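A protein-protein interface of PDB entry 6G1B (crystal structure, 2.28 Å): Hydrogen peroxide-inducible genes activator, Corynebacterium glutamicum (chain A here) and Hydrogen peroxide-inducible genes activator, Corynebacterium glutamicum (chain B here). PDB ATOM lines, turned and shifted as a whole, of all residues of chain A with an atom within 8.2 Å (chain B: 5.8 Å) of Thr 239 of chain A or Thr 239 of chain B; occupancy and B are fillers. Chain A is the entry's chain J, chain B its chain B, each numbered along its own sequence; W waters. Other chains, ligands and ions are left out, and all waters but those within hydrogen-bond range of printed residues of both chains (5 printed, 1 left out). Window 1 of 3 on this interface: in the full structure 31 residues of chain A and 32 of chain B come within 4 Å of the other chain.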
ATOM      1  N   PRO A 109      38.602 -20.842  32.374  1.00  0.00           N
ATOM      2  CA  PRO A 109      37.586 -20.521  31.348  1.00  0.00           C
ATOM      3  C   PRO A 109      36.354 -19.733  31.823  1.00  0.00           C
ATOM      4  O   PRO A 109      35.743 -19.052  31.006  1.00  0.00           O
ATOM      5  CB  PRO A 109      37.140 -21.899  30.831  1.00  0.00           C
ATOM      6  CG  PRO A 109      38.145 -22.864  31.322  1.00  0.00           C
ATOM      7  CD  PRO A 109      38.716 -22.299  32.573  1.00  0.00           C
ATOM      8  N   THR A 110      35.974 -19.840  33.093  1.00  0.00           N
ATOM      9  CA  THR A 110      34.809 -19.086  33.602  1.00  0.00           C
ATOM     10  C   THR A 110      35.135 -17.682  34.109  1.00  0.00           C
ATOM     11  O   THR A 110      34.255 -16.996  34.622  1.00  0.00           O
ATOM     12  CB  THR A 110      34.076 -19.866  34.715  1.00  0.00           C
ATOM     13  OG1 THR A 110      34.978 -20.193  35.776  1.00  0.00           O
ATOM     14  CG2 THR A 110      33.468 -21.159  34.128  1.00  0.00           C
ATOM     15  N   ALA A 112      38.155 -15.877  32.265  1.00  0.00           N
ATOM     16  CA  ALA A 112      38.795 -15.286  31.099  1.00  0.00           C
ATOM     17  C   ALA A 112      37.919 -14.416  30.180  1.00  0.00           C
ATOM     18  O   ALA A 112      38.296 -13.287  29.941  1.00  0.00           O
ATOM     19  CB  ALA A 112      39.534 -16.354  30.294  1.00  0.00           C
ATOM     20  N   PRO A 113      36.764 -14.902  29.691  1.00  0.00           N
ATOM     21  CA  PRO A 113      36.022 -14.136  28.666  1.00  0.00           C
ATOM     22  C   PRO A 113      35.535 -12.764  29.116  1.00  0.00           C
ATOM     23  O   PRO A 113      35.472 -11.810  28.310  1.00  0.00           O
ATOM     24  CB  PRO A 113      34.818 -15.017  28.342  1.00  0.00           C
ATOM     25  CG  PRO A 113      35.087 -16.351  28.965  1.00  0.00           C
ATOM     26  CD  PRO A 113      36.042 -16.110  30.094  1.00  0.00           C
ATOM     27  N   TYR A 114      35.268 -12.658  30.409  1.00  0.00           N
ATOM     28  CA  TYR A 114      34.562 -11.537  30.970  1.00  0.00           C
ATOM     29  C   TYR A 114      35.526 -10.430  31.465  1.00  0.00           C
ATOM     30  O   TYR A 114      35.072  -9.261  31.636  1.00  0.00           O
ATOM     31  CB  TYR A 114      33.616 -12.041  32.055  1.00  0.00           C
ATOM     32  CG  TYR A 114      32.893 -13.312  31.630  1.00  0.00           C
ATOM     33  CD1 TYR A 114      31.994 -13.291  30.564  1.00  0.00           C
ATOM     34  CD2 TYR A 114      33.153 -14.538  32.251  1.00  0.00           C
ATOM     35  CE1 TYR A 114      31.351 -14.440  30.121  1.00  0.00           C
ATOM     36  CE2 TYR A 114      32.514 -15.693  31.836  1.00  0.00           C
ATOM     37  CZ  TYR A 114      31.618 -15.653  30.746  1.00  0.00           C
ATOM     38  OH  TYR A 114      30.964 -16.815  30.310  1.00  0.00           O
ATOM     39  N   LEU A 116      39.041 -10.454  30.007  1.00  0.00           N
ATOM     40  CA  LEU A 116      40.243 -10.471  29.124  1.00  0.00           C
ATOM     41  C   LEU A 116      40.355  -9.188  28.279  1.00  0.00           C
ATOM     42  O   LEU A 116      41.419  -8.599  28.220  1.00  0.00           O
ATOM     43  CB  LEU A 116      40.308 -11.755  28.304  1.00  0.00           C
ATOM     44  CG  LEU A 116      41.583 -12.137  27.564  1.00  0.00           C
ATOM     45  CD1 LEU A 116      42.838 -11.924  28.403  1.00  0.00           C
ATOM     46  CD2 LEU A 116      41.520 -13.566  27.092  1.00  0.00           C
ATOM     47  N   PRO A 117      39.238  -8.719  27.683  1.00  0.00           N
ATOM     48  CA  PRO A 117      39.306  -7.465  26.946  1.00  0.00           C
ATOM     49  C   PRO A 117      39.715  -6.245  27.758  1.00  0.00           C
ATOM     50  O   PRO A 117      40.543  -5.480  27.271  1.00  0.00           O
ATOM     51  CB  PRO A 117      37.908  -7.319  26.368  1.00  0.00           C
ATOM     52  CG  PRO A 117      37.449  -8.720  26.241  1.00  0.00           C
ATOM     53  CD  PRO A 117      37.937  -9.372  27.486  1.00  0.00           C
ATOM     54  N   GLU A 136      44.246 -19.875  28.061  1.00  0.00           N
ATOM     55  CA  GLU A 136      42.991 -20.146  28.744  1.00  0.00           C
ATOM     56  C   GLU A 136      42.759 -21.648  28.767  1.00  0.00           C
ATOM     57  O   GLU A 136      42.708 -22.271  27.714  1.00  0.00           O
ATOM     58  CB  GLU A 136      41.847 -19.428  28.044  1.00  0.00           C
ATOM     59  CG  GLU A 136      40.488 -19.601  28.722  1.00  0.00           C
ATOM     60  CD  GLU A 136      39.340 -19.845  27.773  1.00  0.00           C
ATOM     61  OE1 GLU A 136      39.492 -19.958  26.563  1.00  0.00           O
ATOM     62  OE2 GLU A 136      38.218 -19.889  28.234  1.00  0.00           O
ATOM     63  N   LEU A 204      28.921 -25.753  37.281  1.00  0.00           N
ATOM     64  CA  LEU A 204      30.257 -25.929  36.752  1.00  0.00           C
ATOM     65  C   LEU A 204      31.278 -25.913  37.868  1.00  0.00           C
ATOM     66  O   LEU A 204      31.024 -25.365  38.948  1.00  0.00           O
ATOM     67  CB  LEU A 204      30.574 -24.753  35.834  1.00  0.00           C
ATOM     68  CG  LEU A 204      29.703 -24.648  34.582  1.00  0.00           C
ATOM     69  CD1 LEU A 204      30.127 -23.435  33.780  1.00  0.00           C
ATOM     70  CD2 LEU A 204      29.804 -25.906  33.721  1.00  0.00           C
ATOM     71  N   ALA A 235      28.821 -30.543  32.582  1.00  0.00           N
ATOM     72  CA  ALA A 235      29.259 -29.688  31.514  1.00  0.00           C
ATOM     73  C   ALA A 235      30.581 -29.054  31.908  1.00  0.00           C
ATOM     74  O   ALA A 235      30.856 -28.849  33.051  1.00  0.00           O
ATOM     75  CB  ALA A 235      28.194 -28.624  31.296  1.00  0.00           C
ATOM     76  N   SER A 236      31.430 -28.750  30.946  1.00  0.00           N
ATOM     77  CA  SER A 236      32.622 -27.924  31.201  1.00  0.00           C
ATOM     78  C   SER A 236      32.426 -26.486  30.752  1.00  0.00           C
ATOM     79  O   SER A 236      33.222 -25.631  31.097  1.00  0.00           O
ATOM     80  CB  SER A 236      33.844 -28.532  30.503  1.00  0.00           C
ATOM     81  OG  SER A 236      33.824 -28.331  29.089  1.00  0.00           O
ATOM     82  N   SER A 237      31.374 -26.219  29.974  1.00  0.00           N
ATOM     83  CA  SER A 237      31.101 -24.917  29.441  1.00  0.00           C
ATOM     84  C   SER A 237      29.757 -24.365  29.944  1.00  0.00           C
ATOM     85  O   SER A 237      28.736 -25.049  29.958  1.00  0.00           O
ATOM     86  CB  SER A 237      31.062 -25.018  27.933  1.00  0.00           C
ATOM     87  OG  SER A 237      30.721 -23.762  27.395  1.00  0.00           O
ATOM     88  N   LEU A 238      29.781 -23.092  30.317  1.00  0.00           N
ATOM     89  CA  LEU A 238      28.583 -22.338  30.654  1.00  0.00           C
ATOM     90  C   LEU A 238      27.561 -22.268  29.514  1.00  0.00           C
ATOM     91  O   LEU A 238      26.359 -22.170  29.775  1.00  0.00           O
ATOM     92  CB  LEU A 238      28.984 -20.913  31.081  1.00  0.00           C
ATOM     93  CG  LEU A 238      27.911 -20.055  31.743  1.00  0.00           C
ATOM     94  CD1 LEU A 238      27.273 -20.792  32.921  1.00  0.00           C
ATOM     95  CD2 LEU A 238      28.536 -18.758  32.237  1.00  0.00           C
ATOM     96  N   THR A 239      28.013 -22.322  28.263  1.00  0.00           N
ATOM     97  CA  THR A 239      27.151 -22.301  27.097  1.00  0.00           C
ATOM     98  C   THR A 239      26.209 -23.518  27.036  1.00  0.00           C
ATOM     99  O   THR A 239      25.045 -23.386  26.755  1.00  0.00           O
ATOM    100  CB  THR A 239      28.007 -22.148  25.822  1.00  0.00           C
ATOM    101  OG1 THR A 239      28.797 -20.950  25.940  1.00  0.00           O
ATOM    102  CG2 THR A 239      27.157 -22.101  24.560  1.00  0.00           C
ATOM    103  N   THR A 240      26.742 -24.697  27.288  1.00  0.00           N
ATOM    104  CA  THR A 240      25.957 -25.918  27.411  1.00  0.00           C
ATOM    105  C   THR A 240      24.885 -25.768  28.528  1.00  0.00           C
ATOM    106  O   THR A 240      23.713 -26.064  28.307  1.00  0.00           O
ATOM    107  CB  THR A 240      26.871 -27.119  27.707  1.00  0.00           C
ATOM    108  OG1 THR A 240      27.765 -27.317  26.604  1.00  0.00           O
ATOM    109  CG2 THR A 240      26.058 -28.388  27.925  1.00  0.00           C
ATOM    110  N   VAL A 241      25.297 -25.246  29.680  1.00  0.00           N
ATOM    111  CA  VAL A 241      24.393 -25.025  30.812  1.00  0.00           C
ATOM    112  C   VAL A 241      23.254 -24.010  30.480  1.00  0.00           C
ATOM    113  O   VAL A 241      22.073 -24.296  30.723  1.00  0.00           O
ATOM    114  CB  VAL A 241      25.208 -24.602  32.069  1.00  0.00           C
ATOM    115  CG1 VAL A 241      24.295 -24.161  33.223  1.00  0.00           C
ATOM    116  CG2 VAL A 241      26.192 -25.714  32.479  1.00  0.00           C
ATOM    117  N   MET A 242      23.620 -22.858  29.904  1.00  0.00           N
ATOM    118  CA  MET A 242      22.633 -21.839  29.543  1.00  0.00           C
ATOM    119  C   MET A 242      21.614 -22.330  28.535  1.00  0.00           C
ATOM    120  O   MET A 242      20.436 -21.962  28.604  1.00  0.00           O
ATOM    121  CB  MET A 242      23.290 -20.589  28.975  1.00  0.00           C
ATOM    122  CG  MET A 242      24.100 -19.823  29.995  1.00  0.00           C
ATOM    123  SD  MET A 242      23.026 -19.234  31.339  1.00  0.00           S
ATOM    124  CE  MET A 242      24.113 -19.719  32.626  1.00  0.00           C
ATOM    125  N   GLN A 243      22.077 -23.122  27.577  1.00  0.00           N
ATOM    126  CA  GLN A 243      21.197 -23.815  26.660  1.00  0.00           C
ATOM    127  C   GLN A 243      20.121 -24.622  27.383  1.00  0.00           C
ATOM    128  O   GLN A 243      18.933 -24.530  27.059  1.00  0.00           O
ATOM    129  CB  GLN A 243      22.011 -24.795  25.798  1.00  0.00           C
ATOM    130  CG  GLN A 243      21.471 -24.888  24.436  1.00  0.00           C
ATOM    131  CD  GLN A 243      21.823 -23.686  23.648  1.00  0.00           C
ATOM    132  OE1 GLN A 243      21.070 -23.282  22.776  1.00  0.00           O
ATOM    133  NE2 GLN A 243      22.986 -23.108  23.938  1.00  0.00           N
ATOM    134  N   LEU A 244      20.559 -25.415  28.351  1.00  0.00           N
ATOM    135  CA  LEU A 244      19.647 -26.220  29.153  1.00  0.00           C
ATOM    136  C   LEU A 244      18.708 -25.369  30.013  1.00  0.00           C
ATOM    137  O   LEU A 244      17.540 -25.706  30.144  1.00  0.00           O
ATOM    138  CB  LEU A 244      20.449 -27.196  30.021  1.00  0.00           C
ATOM    139  CG  LEU A 244      21.139 -28.243  29.138  1.00  0.00           C
ATOM    140  CD1 LEU A 244      22.371 -28.823  29.765  1.00  0.00           C
ATOM    141  CD2 LEU A 244      20.144 -29.331  28.824  1.00  0.00           C
ATOM    142  N   VAL A 245      19.209 -24.252  30.547  1.00  0.00           N
ATOM    143  CA  VAL A 245      18.381 -23.326  31.333  1.00  0.00           C
ATOM    144  C   VAL A 245      17.297 -22.635  30.492  1.00  0.00           C
ATOM    145  O   VAL A 245      16.135 -22.575  30.928  1.00  0.00           O
ATOM    146  CB  VAL A 245      19.217 -22.259  32.081  1.00  0.00           C
ATOM    147  CG1 VAL A 245      18.322 -21.238  32.774  1.00  0.00           C
ATOM    148  CG2 VAL A 245      20.139 -22.894  33.136  1.00  0.00           C
ATOM    149  N   VAL A 246      17.653 -22.123  29.312  1.00  0.00           N
ATOM    150  CA  VAL A 246      16.676 -21.512  28.401  1.00  0.00           C
ATOM    151  C   VAL A 246      15.592 -22.523  28.046  1.00  0.00           C
ATOM    152  O   VAL A 246      14.408 -22.169  28.034  1.00  0.00           O
ATOM    153  CB  VAL A 246      17.338 -21.023  27.087  1.00  0.00           C
ATOM    154  CG1 VAL A 246      16.321 -20.752  25.972  1.00  0.00           C
ATOM    155  CG2 VAL A 246      18.178 -19.784  27.370  1.00  0.00           C
ATOM    156  N   ALA A 258      30.043 -12.324  34.281  1.00  0.00           N
ATOM    157  CA  ALA A 258      29.462 -12.913  33.087  1.00  0.00           C
ATOM    158  C   ALA A 258      28.049 -12.425  32.800  1.00  0.00           C
ATOM    159  O   ALA A 258      27.458 -12.868  31.843  1.00  0.00           O
ATOM    160  CB  ALA A 258      29.462 -14.425  33.200  1.00  0.00           C
ATOM    161  N   TRP A 261      27.286 -10.638  29.180  1.00  0.00           N
ATOM    162  CA  TRP A 261      27.423 -11.544  28.049  1.00  0.00           C
ATOM    163  C   TRP A 261      26.415 -12.689  28.078  1.00  0.00           C
ATOM    164  O   TRP A 261      25.899 -13.045  27.053  1.00  0.00           O
ATOM    165  CB  TRP A 261      28.853 -12.100  27.993  1.00  0.00           C
ATOM    166  CG  TRP A 261      29.146 -12.906  26.749  1.00  0.00           C
ATOM    167  CD1 TRP A 261      28.960 -14.234  26.579  1.00  0.00           C
ATOM    168  CD2 TRP A 261      29.706 -12.420  25.529  1.00  0.00           C
ATOM    169  NE1 TRP A 261      29.352 -14.617  25.335  1.00  0.00           N
ATOM    170  CE2 TRP A 261      29.813 -13.518  24.661  1.00  0.00           C
ATOM    171  CE3 TRP A 261      30.116 -11.156  25.078  1.00  0.00           C
ATOM    172  CZ2 TRP A 261      30.332 -13.396  23.360  1.00  0.00           C
ATOM    173  CZ3 TRP A 261      30.601 -11.033  23.808  1.00  0.00           C
ATOM    174  CH2 TRP A 261      30.715 -12.135  22.958  1.00  0.00           C
ATOM    175  N   GLU A 262      26.180 -13.266  29.255  1.00  0.00           N
ATOM    176  CA  GLU A 262      25.408 -14.532  29.420  1.00  0.00           C
ATOM    177  C   GLU A 262      23.961 -14.382  29.852  1.00  0.00           C
ATOM    178  O   GLU A 262      23.126 -15.214  29.476  1.00  0.00           O
ATOM    179  CB  GLU A 262      26.092 -15.471  30.432  1.00  0.00           C
ATOM    180  CG  GLU A 262      27.554 -15.783  30.150  1.00  0.00           C
ATOM    181  CD  GLU A 262      27.780 -16.736  29.000  1.00  0.00           C
ATOM    182  OE1 GLU A 262      26.804 -17.140  28.295  1.00  0.00           O
ATOM    183  OE2 GLU A 262      28.981 -17.092  28.799  1.00  0.00           O
ATOM    184  N   ARG A 265      20.131 -12.312  27.348  1.00  0.00           N
ATOM    185  CA  ARG A 265      19.367 -12.912  26.267  1.00  0.00           C
ATOM    186  C   ARG A 265      17.935 -13.320  26.697  1.00  0.00           C
ATOM    187  O   ARG A 265      17.687 -13.599  27.867  1.00  0.00           O
ATOM    188  CB  ARG A 265      20.136 -14.133  25.729  1.00  0.00           C
ATOM    189  CG  ARG A 265      20.243 -15.280  26.710  1.00  0.00           C
ATOM    190  CD  ARG A 265      20.963 -16.503  26.186  1.00  0.00           C
ATOM    191  NE  ARG A 265      22.236 -16.314  25.490  1.00  0.00           N
ATOM    192  CZ  ARG A 265      22.415 -16.396  24.172  1.00  0.00           C
ATOM    193  NH1 ARG A 265      21.399 -16.583  23.336  1.00  0.00           N
ATOM    194  NH2 ARG A 265      23.620 -16.253  23.680  1.00  0.00           N
ATOM    195  N   PRO B 113      26.335 -27.667  22.997  1.00  0.00           N
ATOM    196  CA  PRO B 113      25.285 -26.678  23.300  1.00  0.00           C
ATOM    197  C   PRO B 113      24.268 -26.468  22.172  1.00  0.00           C
ATOM    198  O   PRO B 113      23.091 -26.179  22.442  1.00  0.00           O
ATOM    199  CB  PRO B 113      26.052 -25.383  23.502  1.00  0.00           C
ATOM    200  CG  PRO B 113      27.493 -25.760  23.643  1.00  0.00           C
ATOM    201  CD  PRO B 113      27.663 -27.037  22.896  1.00  0.00           C
ATOM    202  N   TYR B 114      24.721 -26.665  20.935  1.00  0.00           N
ATOM    203  CA  TYR B 114      23.977 -26.266  19.760  1.00  0.00           C
ATOM    204  C   TYR B 114      23.085 -27.383  19.202  1.00  0.00           C
ATOM    205  O   TYR B 114      22.131 -27.099  18.477  1.00  0.00           O
ATOM    206  CB  TYR B 114      24.977 -25.729  18.702  1.00  0.00           C
ATOM    207  CG  TYR B 114      26.008 -24.846  19.341  1.00  0.00           C
ATOM    208  CD1 TYR B 114      25.653 -23.632  19.927  1.00  0.00           C
ATOM    209  CD2 TYR B 114      27.342 -25.227  19.397  1.00  0.00           C
ATOM    210  CE1 TYR B 114      26.601 -22.823  20.546  1.00  0.00           C
ATOM    211  CE2 TYR B 114      28.294 -24.421  20.020  1.00  0.00           C
ATOM    212  CZ  TYR B 114      27.912 -23.229  20.610  1.00  0.00           C
ATOM    213  OH  TYR B 114      28.870 -22.415  21.221  1.00  0.00           O
ATOM    214  N   SER B 237      38.027 -21.990  25.110  1.00  0.00           N
ATOM    215  CA  SER B 237      36.582 -21.765  25.026  1.00  0.00           C
ATOM    216  C   SER B 237      36.203 -20.779  23.927  1.00  0.00           C
ATOM    217  O   SER B 237      36.832 -19.755  23.789  1.00  0.00           O
ATOM    218  CB  SER B 237      36.019 -21.274  26.372  1.00  0.00           C
ATOM    219  OG  SER B 237      35.672 -19.881  26.410  1.00  0.00           O
ATOM    220  N   LEU B 238      35.132 -21.083  23.204  1.00  0.00           N
ATOM    221  CA  LEU B 238      34.559 -20.187  22.214  1.00  0.00           C
ATOM    222  C   LEU B 238      34.124 -18.809  22.774  1.00  0.00           C
ATOM    223  O   LEU B 238      34.218 -17.788  22.056  1.00  0.00           O
ATOM    224  CB  LEU B 238      33.385 -20.864  21.500  1.00  0.00           C
ATOM    225  CG  LEU B 238      32.848 -20.159  20.251  1.00  0.00           C
ATOM    226  CD1 LEU B 238      33.951 -19.969  19.235  1.00  0.00           C
ATOM    227  CD2 LEU B 238      31.695 -20.896  19.618  1.00  0.00           C
ATOM    228  N   THR B 239      33.693 -18.789  24.044  1.00  0.00           N
ATOM    229  CA  THR B 239      33.203 -17.560  24.643  1.00  0.00           C
ATOM    230  C   THR B 239      34.354 -16.558  24.842  1.00  0.00           C
ATOM    231  O   THR B 239      34.188 -15.366  24.590  1.00  0.00           O
ATOM    232  CB  THR B 239      32.481 -17.875  25.968  1.00  0.00           C
ATOM    233  OG1 THR B 239      31.397 -18.781  25.707  1.00  0.00           O
ATOM    234  CG2 THR B 239      31.945 -16.613  26.635  1.00  0.00           C
ATOM    235  N   THR B 240      35.502 -17.045  25.297  1.00  0.00           N
ATOM    236  CA  THR B 240      36.713 -16.237  25.376  1.00  0.00           C
ATOM    237  C   THR B 240      37.069 -15.623  24.005  1.00  0.00           C
ATOM    238  O   THR B 240      37.312 -14.443  23.913  1.00  0.00           O
ATOM    239  CB  THR B 240      37.888 -17.091  25.918  1.00  0.00           C
ATOM    240  OG1 THR B 240      37.595 -17.439  27.273  1.00  0.00           O
ATOM    241  CG2 THR B 240      39.185 -16.349  25.891  1.00  0.00           C
ATOM    242  N   VAL B 241      37.026 -16.442  22.959  1.00  0.00           N
ATOM    243  CA  VAL B 241      37.348 -16.011  21.604  1.00  0.00           C
ATOM    244  C   VAL B 241      36.345 -14.947  21.082  1.00  0.00           C
ATOM    245  O   VAL B 241      36.746 -13.913  20.579  1.00  0.00           O
ATOM    246  CB  VAL B 241      37.452 -17.252  20.661  1.00  0.00           C
ATOM    247  CG1 VAL B 241      37.609 -16.853  19.227  1.00  0.00           C
ATOM    248  CG2 VAL B 241      38.636 -18.110  21.057  1.00  0.00           C
ATOM    249  N   MET B 242      35.053 -15.191  21.224  1.00  0.00           N
ATOM    250  CA  MET B 242      34.050 -14.234  20.766  1.00  0.00           C
ATOM    251  C   MET B 242      34.134 -12.869  21.461  1.00  0.00           C
ATOM    252  O   MET B 242      33.924 -11.815  20.839  1.00  0.00           O
ATOM    253  CB  MET B 242      32.651 -14.769  20.970  1.00  0.00           C
ATOM    254  CG  MET B 242      32.304 -16.011  20.183  1.00  0.00           C
ATOM    255  SD  MET B 242      32.661 -15.901  18.432  1.00  0.00           S
ATOM    256  CE  MET B 242      31.363 -14.796  17.936  1.00  0.00           C
ATOM    257  N   GLN B 243      34.424 -12.905  22.752  1.00  0.00           N
ATOM    258  CA  GLN B 243      34.697 -11.685  23.493  1.00  0.00           C
ATOM    259  C   GLN B 243      35.887 -10.907  22.878  1.00  0.00           C
ATOM    260  O   GLN B 243      35.836  -9.717  22.724  1.00  0.00           O
ATOM    261  CB  GLN B 243      34.918 -11.964  24.994  1.00  0.00           C
ATOM    262  CG  GLN B 243      33.635 -12.159  25.767  1.00  0.00           C
ATOM    263  CD  GLN B 243      33.227 -10.988  26.650  1.00  0.00           C
ATOM    264  OE1 GLN B 243      33.410  -9.808  26.321  1.00  0.00           O
ATOM    265  NE2 GLN B 243      32.644 -11.320  27.778  1.00  0.00           N
ATOM    266  N   LEU B 244      36.934 -11.607  22.535  1.00  0.00           N
ATOM    267  CA  LEU B 244      38.108 -11.006  21.886  1.00  0.00           C
ATOM    268  C   LEU B 244      37.793 -10.480  20.497  1.00  0.00           C
ATOM    269  O   LEU B 244      38.277  -9.419  20.130  1.00  0.00           O
ATOM    270  CB  LEU B 244      39.267 -12.013  21.826  1.00  0.00           C
ATOM    271  CG  LEU B 244      39.759 -12.390  23.217  1.00  0.00           C
ATOM    272  CD1 LEU B 244      40.576 -13.642  23.121  1.00  0.00           C
ATOM    273  CD2 LEU B 244      40.581 -11.282  23.856  1.00  0.00           C
ATOM    274  N   TRP B 261      23.160 -18.952  18.406  1.00  0.00           N
ATOM    275  CA  TRP B 261      23.533 -18.631  19.776  1.00  0.00           C
ATOM    276  C   TRP B 261      24.690 -17.644  19.850  1.00  0.00           C
ATOM    277  O   TRP B 261      24.647 -16.741  20.691  1.00  0.00           O
ATOM    278  CB  TRP B 261      23.884 -19.897  20.553  1.00  0.00           C
ATOM    279  CG  TRP B 261      24.093 -19.674  22.027  1.00  0.00           C
ATOM    280  CD1 TRP B 261      25.259 -19.309  22.665  1.00  0.00           C
ATOM    281  CD2 TRP B 261      23.115 -19.813  23.054  1.00  0.00           C
ATOM    282  NE1 TRP B 261      25.056 -19.211  24.014  1.00  0.00           N
ATOM    283  CE2 TRP B 261      23.757 -19.539  24.285  1.00  0.00           C
ATOM    284  CE3 TRP B 261      21.770 -20.191  23.062  1.00  0.00           C
ATOM    285  CZ2 TRP B 261      23.076 -19.577  25.504  1.00  0.00           C
ATOM    286  CZ3 TRP B 261      21.104 -20.251  24.268  1.00  0.00           C
ATOM    287  CH2 TRP B 261      21.747 -19.929  25.471  1.00  0.00           C
ATOM    288  N   GLU B 262      25.708 -17.820  18.998  1.00  0.00           N
ATOM    289  CA  GLU B 262      26.990 -17.066  19.112  1.00  0.00           C
ATOM    290  C   GLU B 262      27.144 -15.866  18.177  1.00  0.00           C
ATOM    291  O   GLU B 262      27.849 -14.916  18.521  1.00  0.00           O
ATOM    292  CB  GLU B 262      28.195 -17.991  18.853  1.00  0.00           C
ATOM    293  CG  GLU B 262      28.281 -19.248  19.691  1.00  0.00           C
ATOM    294  CD  GLU B 262      28.635 -18.998  21.164  1.00  0.00           C
ATOM    295  OE1 GLU B 262      28.825 -17.817  21.596  1.00  0.00           O
ATOM    296  OE2 GLU B 262      28.717 -20.006  21.905  1.00  0.00           O
HETATM  297  O   HOH W   1      29.018 -17.135  24.163  1.00  0.00           O
HETATM  298  O   HOH W   2      30.079 -19.199  27.917  1.00  0.00           O
HETATM  299  O   HOH W   3      34.518 -19.821  28.744  1.00  0.00           O
HETATM  300  O   HOH W   4      30.328 -20.663  23.760  1.00  0.00           O
HETATM  301  O   HOH W   5      27.118 -18.260  25.866  1.00  0.00           O
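The backbone carbonyl oxygen (O) of Pro 113 of chain A sits close to the side-chain amide nitrogen (NE2) of Gln 243 of chain B, at 2.9 Å.
OE1 of Glu 136 of chain A sits at hydrogen-bond distance from N of Ser 237 of chain B (2.9 Å).
The side-chain carboxylate of Glu 136 of chain A is in hydrogen-bond range of the side-chain hydroxyl of Thr 240 of chain B, at 2.7 Å.
OG1 of Thr 239 of chain B is in hydrogen-bond range of OG1 of Thr 239 of chain A (3.4 Å).
The side-chain amide nitrogen (NE2) of Gln 243 of chain A sits close to the backbone carbonyl oxygen (O) of Pro 113 of chain B (3.4 Å).
The guanidinium group of Arg 265 of chain A is in hydrogen-bond range of the backbone carbonyl oxygen of Trp 261 of chain B (3.2 Å).
Water W4 lies within hydrogen-bond range of OE2 of Glu 262 of chain B (2.5 Å), OG1 of Thr 239 of chain A (2.7 Å), OG1 of Thr 239 of chain B (2.9 Å) and OH of Tyr 114 of chain B (3.4 Å).
Water W5 lies within hydrogen-bond range of the side-chain carboxylate (OE1) of Glu 262 of chain A (2.7 Å), the indole nitrogen (NE1) of Trp 261 of chain B (2.9 Å) and the side-chain hydroxyl (OG1) of Thr 239 of chain A (3.2 Å).
Of the 12 printed residues of chain B, 10 touch a printed residue of chain A.
Printed residues of chain B that touch a printed residue of chain A: Pro 113, Tyr 114, Ser 237, Thr 239, Thr 240, Met 242, Gln 243, Leu 244, Trp 261 and Glu 262.
Of the 25 printed residues of chain A, 13 touch a printed residue of chain B.
Hydrophobic or aromatic side chains of chain A within 4 Å of the printed part of chain B: Ala 112, Pro 113, Tyr 114, Leu 116, Pro 117, Met 242 and Trp 261.
Along chain A the printed residues that touch a printed residue of chain B span positions 112 to 265.
Among the printed residues, pairs that only touch across the chains: Gln 243 of chain A with Trp 261 of chain B, Pro 113 of chain A with Thr 240 of chain B, Thr 240 of chain A with Pro 113 of chain B, Tyr 114 of chain A with Gln 243 of chain B, Trp 261 of chain A with Gln 243 of chain B, Trp 261 of chain A with Thr 239 of chain B, Trp 261 of chain A with Met 242 of chain B, Thr 239 of chain A with Trp 261 of chain B, Thr 239 of chain A with Pro 113 of chain B, Met 242 of chain A with Trp 261 of chain B, Glu 262 of chain A with Thr 239 of chain B, Pro 113 of chain A with Thr 239 of chain B, Thr 239 of chain A with Glu 262 of chain B, Ala 112 of chain A with Thr 240 of chain B, Thr 239 of chain A with Tyr 114 of chain B, Tyr 114 of chain A with Thr 239 of chain B, Leu 116 of chain A with Thr 240 of chain B, Leu 116 of chain A with Leu 244 of chain B and Pro 117 of chain A with Gln 243 of chain B.
The side-chain hydroxyl of Tyr 114 of chain A sits at hydrogen-bond distance from the side-chain carboxylate of Glu 262 of chain A.
The side-chain hydroxyl (OG) of Ser 237 of chain A sits close to the backbone NH (N) of Thr 239 of chain A, at 3.2 Å.
The side-chain carboxylate of Glu 262 of chain B sits at hydrogen-bond distance from the side-chain hydroxyl of Tyr 114 of chain B.
Of chain B, only Pro 113, Tyr 114, Thr 239, Trp 261 and Glu 262 come within 4 Å of Thr 239 of chain A.
Of chain A, only Pro 113, Tyr 114, Thr 239, Trp 261 and Glu 262 come within 4 Å of Thr 239 of chain B.
Of the printed residues of chain B, Pro 117 of chain A touches Gln 243.
Of the printed residues of chain B, Gln 243 of chain A touches Pro 113 and Trp 261.
Of the printed residues of chain B, Leu 116 of chain A touches Thr 240 and Leu 244.
Leu 238 of chain B touches none of the printed residues of chain A.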
